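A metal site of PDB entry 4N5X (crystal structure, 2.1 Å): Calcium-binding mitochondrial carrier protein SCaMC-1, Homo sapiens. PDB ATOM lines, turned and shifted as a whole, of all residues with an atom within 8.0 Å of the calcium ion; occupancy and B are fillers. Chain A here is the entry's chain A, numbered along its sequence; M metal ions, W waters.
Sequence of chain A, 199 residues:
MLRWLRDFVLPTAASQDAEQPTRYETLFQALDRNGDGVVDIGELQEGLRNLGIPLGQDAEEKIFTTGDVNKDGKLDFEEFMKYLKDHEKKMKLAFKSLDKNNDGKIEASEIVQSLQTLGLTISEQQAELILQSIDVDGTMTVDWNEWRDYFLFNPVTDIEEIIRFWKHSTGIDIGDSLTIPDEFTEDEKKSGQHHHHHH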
ATOM      1  N   VAL A  38       4.565 -10.309  20.156  1.00  0.00           N
ATOM      2  CA  VAL A  38       3.970 -11.226  21.131  1.00  0.00           C
ATOM      3  C   VAL A  38       4.888 -12.414  21.364  1.00  0.00           C
ATOM      4  O   VAL A  38       5.818 -12.666  20.594  1.00  0.00           O
ATOM      5  CB  VAL A  38       2.585 -11.751  20.681  1.00  0.00           C
ATOM      6  CG1 VAL A  38       1.613 -10.609  20.575  1.00  0.00           C
ATOM      7  CG2 VAL A  38       2.693 -12.486  19.359  1.00  0.00           C
ATOM      8  N   VAL A  39       4.630 -13.128  22.448  1.00  0.00           N
ATOM      9  CA  VAL A  39       5.431 -14.305  22.751  1.00  0.00           C
ATOM     10  C   VAL A  39       4.604 -15.558  22.518  1.00  0.00           C
ATOM     11  O   VAL A  39       3.539 -15.726  23.120  1.00  0.00           O
ATOM     12  CB  VAL A  39       5.968 -14.267  24.198  1.00  0.00           C
ATOM     13  CG1 VAL A  39       6.595 -15.604  24.564  1.00  0.00           C
ATOM     14  CG2 VAL A  39       6.973 -13.126  24.362  1.00  0.00           C
ATOM     15  N   PHE A  64       1.133 -20.768  29.906  1.00  0.00           N
ATOM     16  CA  PHE A  64       0.167 -20.279  28.927  1.00  0.00           C
ATOM     17  C   PHE A  64      -1.270 -20.493  29.393  1.00  0.00           C
ATOM     18  O   PHE A  64      -2.117 -19.638  29.188  1.00  0.00           O
ATOM     19  CB  PHE A  64       0.378 -20.949  27.581  1.00  0.00           C
ATOM     20  CG  PHE A  64       1.089 -20.076  26.600  1.00  0.00           C
ATOM     21  CD1 PHE A  64       2.429 -19.746  26.802  1.00  0.00           C
ATOM     22  CD2 PHE A  64       0.445 -19.579  25.487  1.00  0.00           C
ATOM     23  CE1 PHE A  64       3.112 -18.933  25.905  1.00  0.00           C
ATOM     24  CE2 PHE A  64       1.109 -18.764  24.577  1.00  0.00           C
ATOM     25  CZ  PHE A  64       2.449 -18.445  24.800  1.00  0.00           C
ATOM     26  N   GLY A  67      -1.627 -17.644  31.759  1.00  0.00           N
ATOM     27  CA  GLY A  67      -1.289 -16.328  31.219  1.00  0.00           C
ATOM     28  C   GLY A  67      -2.042 -15.881  29.973  1.00  0.00           C
ATOM     29  O   GLY A  67      -2.337 -14.702  29.828  1.00  0.00           O
ATOM     30  N   ASP A  68      -2.348 -16.823  29.071  1.00  0.00           N
ATOM     31  CA  ASP A  68      -3.011 -16.465  27.810  1.00  0.00           C
ATOM     32  C   ASP A  68      -4.495 -16.268  28.051  1.00  0.00           C
ATOM     33  O   ASP A  68      -5.310 -17.101  27.666  1.00  0.00           O
ATOM     34  CB  ASP A  68      -2.810 -17.554  26.756  1.00  0.00           C
ATOM     35  CG  ASP A  68      -3.399 -17.180  25.405  1.00  0.00           C
ATOM     36  OD1 ASP A  68      -3.827 -16.016  25.227  1.00  0.00           O
ATOM     37  OD2 ASP A  68      -3.453 -18.057  24.519  1.00  0.00           O
ATOM     38  N   VAL A  69      -4.833 -15.164  28.694  1.00  0.00           N
ATOM     39  CA  VAL A  69      -6.192 -14.963  29.168  1.00  0.00           C
ATOM     40  C   VAL A  69      -7.239 -14.972  28.043  1.00  0.00           C
ATOM     41  O   VAL A  69      -8.334 -15.510  28.228  1.00  0.00           O
ATOM     42  CB  VAL A  69      -6.274 -13.690  30.033  1.00  0.00           C
ATOM     43  CG1 VAL A  69      -7.732 -13.243  30.231  1.00  0.00           C
ATOM     44  CG2 VAL A  69      -5.565 -13.929  31.377  1.00  0.00           C
ATOM     45  N   ASN A  70      -6.906 -14.424  26.878  1.00  0.00           N
ATOM     46  CA  ASN A  70      -7.872 -14.369  25.773  1.00  0.00           C
ATOM     47  C   ASN A  70      -7.849 -15.591  24.859  1.00  0.00           C
ATOM     48  O   ASN A  70      -8.604 -15.656  23.882  1.00  0.00           O
ATOM     49  CB  ASN A  70      -7.777 -13.056  24.979  1.00  0.00           C
ATOM     50  CG  ASN A  70      -6.424 -12.854  24.314  1.00  0.00           C
ATOM     51  OD1 ASN A  70      -5.613 -13.764  24.240  1.00  0.00           O
ATOM     52  ND2 ASN A  70      -6.189 -11.645  23.800  1.00  0.00           N
ATOM     53  N   LYS A  71      -7.003 -16.571  25.184  1.00  0.00           N
ATOM     54  CA  LYS A  71      -6.933 -17.818  24.431  1.00  0.00           C
ATOM     55  C   LYS A  71      -6.665 -17.596  22.933  1.00  0.00           C
ATOM     56  O   LYS A  71      -7.123 -18.381  22.111  1.00  0.00           O
ATOM     57  CB  LYS A  71      -8.222 -18.647  24.580  1.00  0.00           C
ATOM     58  CG  LYS A  71      -8.678 -18.889  26.028  1.00  0.00           C
ATOM     59  CD  LYS A  71      -7.916 -20.029  26.686  1.00  0.00           C
ATOM     60  CE  LYS A  71      -8.473 -20.375  28.075  1.00  0.00           C
ATOM     61  NZ  LYS A  71      -9.768 -21.125  28.007  1.00  0.00           N
ATOM     62  N   ASP A  72      -5.932 -16.545  22.581  1.00  0.00           N
ATOM     63  CA  ASP A  72      -5.569 -16.349  21.163  1.00  0.00           C
ATOM     64  C   ASP A  72      -4.247 -17.023  20.767  1.00  0.00           C
ATOM     65  O   ASP A  72      -3.792 -16.898  19.631  1.00  0.00           O
ATOM     66  CB  ASP A  72      -5.564 -14.859  20.784  1.00  0.00           C
ATOM     67  CG  ASP A  72      -4.484 -14.062  21.494  1.00  0.00           C
ATOM     68  OD1 ASP A  72      -3.665 -14.660  22.234  1.00  0.00           O
ATOM     69  OD2 ASP A  72      -4.443 -12.822  21.311  1.00  0.00           O
ATOM     70  N   GLY A  73      -3.624 -17.713  21.730  1.00  0.00           N
ATOM     71  CA  GLY A  73      -2.437 -18.508  21.448  1.00  0.00           C
ATOM     72  C   GLY A  73      -1.127 -17.751  21.578  1.00  0.00           C
ATOM     73  O   GLY A  73      -0.069 -18.273  21.248  1.00  0.00           O
ATOM     74  N   LYS A  74      -1.189 -16.514  22.062  1.00  0.00           N
ATOM     75  CA  LYS A  74      -0.005 -15.685  22.239  1.00  0.00           C
ATOM     76  C   LYS A  74      -0.092 -14.969  23.575  1.00  0.00           C
ATOM     77  O   LYS A  74      -1.173 -14.726  24.085  1.00  0.00           O
ATOM     78  CB  LYS A  74       0.096 -14.626  21.132  1.00  0.00           C
ATOM     79  CG  LYS A  74      -0.317 -15.114  19.737  1.00  0.00           C
ATOM     80  CD  LYS A  74      -0.425 -13.947  18.765  1.00  0.00           C
ATOM     81  CE  LYS A  74      -1.749 -13.950  18.020  1.00  0.00           C
ATOM     82  NZ  LYS A  74      -2.082 -15.299  17.476  1.00  0.00           N
ATOM     83  N   LEU A  75       1.069 -14.645  24.157  1.00  0.00           N
ATOM     84  CA  LEU A  75       1.114 -13.782  25.328  1.00  0.00           C
ATOM     85  C   LEU A  75       1.503 -12.394  24.866  1.00  0.00           C
ATOM     86  O   LEU A  75       2.602 -12.191  24.372  1.00  0.00           O
ATOM     87  CB  LEU A  75       2.172 -14.258  26.343  1.00  0.00           C
ATOM     88  CG  LEU A  75       1.945 -15.524  27.157  1.00  0.00           C
ATOM     89  CD1 LEU A  75       3.145 -15.742  28.099  1.00  0.00           C
ATOM     90  CD2 LEU A  75       0.635 -15.449  27.925  1.00  0.00           C
ATOM     91  N   ASP A  76       0.604 -11.433  25.013  1.00  0.00           N
ATOM     92  CA  ASP A  76       1.000 -10.070  24.757  1.00  0.00           C
ATOM     93  C   ASP A  76       1.705  -9.533  25.996  1.00  0.00           C
ATOM     94  O   ASP A  76       1.812 -10.247  27.007  1.00  0.00           O
ATOM     95  CB  ASP A  76      -0.199  -9.189  24.347  1.00  0.00           C
ATOM     96  CG  ASP A  76      -1.349  -9.287  25.320  1.00  0.00           C
ATOM     97  OD1 ASP A  76      -1.105  -9.242  26.544  1.00  0.00           O
ATOM     98  OD2 ASP A  76      -2.499  -9.428  24.848  1.00  0.00           O
ATOM     99  N   PHE A  77       2.217  -8.318  25.925  1.00  0.00           N
ATOM    100  CA  PHE A  77       2.993  -7.808  27.047  1.00  0.00           C
ATOM    101  C   PHE A  77       2.154  -7.711  28.316  1.00  0.00           C
ATOM    102  O   PHE A  77       2.644  -8.032  29.409  1.00  0.00           O
ATOM    103  CB  PHE A  77       3.651  -6.469  26.726  1.00  0.00           C
ATOM    104  CG  PHE A  77       4.544  -5.991  27.835  1.00  0.00           C
ATOM    105  CD1 PHE A  77       5.809  -6.529  28.003  1.00  0.00           C
ATOM    106  CD2 PHE A  77       4.102  -5.036  28.734  1.00  0.00           C
ATOM    107  CE1 PHE A  77       6.624  -6.109  29.035  1.00  0.00           C
ATOM    108  CE2 PHE A  77       4.907  -4.607  29.766  1.00  0.00           C
ATOM    109  CZ  PHE A  77       6.176  -5.151  29.913  1.00  0.00           C
ATOM    110  N   GLU A  79      -0.449  -9.543  29.193  1.00  0.00           N
ATOM    111  CA  GLU A  79      -0.653 -10.893  29.719  1.00  0.00           C
ATOM    112  C   GLU A  79       0.624 -11.425  30.397  1.00  0.00           C
ATOM    113  O   GLU A  79       0.569 -12.062  31.443  1.00  0.00           O
ATOM    114  CB  GLU A  79      -1.101 -11.847  28.608  1.00  0.00           C
ATOM    115  CG  GLU A  79      -2.529 -11.636  28.113  1.00  0.00           C
ATOM    116  CD  GLU A  79      -2.841 -12.469  26.887  1.00  0.00           C
ATOM    117  OE1 GLU A  79      -1.918 -12.677  26.080  1.00  0.00           O
ATOM    118  OE2 GLU A  79      -3.995 -12.932  26.738  1.00  0.00           O
ATOM    119  N   PHE A  80       1.758 -11.145  29.770  1.00  0.00           N
ATOM    120  CA  PHE A  80       3.075 -11.561  30.233  1.00  0.00           C
ATOM    121  C   PHE A  80       3.344 -10.936  31.587  1.00  0.00           C
ATOM    122  O   PHE A  80       3.692 -11.624  32.553  1.00  0.00           O
ATOM    123  CB  PHE A  80       4.130 -11.125  29.198  1.00  0.00           C
ATOM    124  CG  PHE A  80       5.545 -11.450  29.572  1.00  0.00           C
ATOM    125  CD1 PHE A  80       6.051 -12.743  29.432  1.00  0.00           C
ATOM    126  CD2 PHE A  80       6.398 -10.448  30.037  1.00  0.00           C
ATOM    127  CE1 PHE A  80       7.358 -13.037  29.768  1.00  0.00           C
ATOM    128  CE2 PHE A  80       7.712 -10.735  30.373  1.00  0.00           C
ATOM    129  CZ  PHE A  80       8.207 -12.029  30.241  1.00  0.00           C
HETATM  130 CA    CA M   1      -3.261 -13.915  24.431  1.00  0.00          CA
HETATM  131  O   HOH W   1      -3.007 -11.667  23.505  1.00  0.00           O
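Water W1 lies within hydrogen-bond range of OD2 of Asp 76, OD2 of Asp 72 and ND2 of Asn 70.
The calcium ion is bound by the backbone carbonyl oxygen (O) of Lys 74 (2.3 Å), the side-chain carboxylate (OD1) of Asp 68 (2.3 Å), the side-chain carboxylate (OD1) of Asp 72 (2.4 Å), the side-chain amide oxygen (OD1) of Asn 70 (2.4 Å), water W1 (2.4 Å), the side-chain carboxylate (OE1) of Glu 79 (2.5 Å) and the side-chain carboxylate (OE2) of Glu 79 (2.6 Å).
The side-chain carboxylate (OD1) of Asp 68 lies close to the backbone NH (N) of Lys 71. The side-chain carboxylate (OD2) of Asp 68 sits at hydrogen-bond distance from the backbone NH (N) of Gly 73. OD1 of Asp 76 is in hydrogen-bond range of N of Glu 79 (2.7 Å). The side-chain carboxylate (OE2) of Glu 79 lies close to the backbone NH (N) of Val 69 (3.1 Å).
Five residues have an atom within 4 Å of the calcium ion: Asp 68, Asn 70, Asp 72, Lys 74 and Glu 79.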
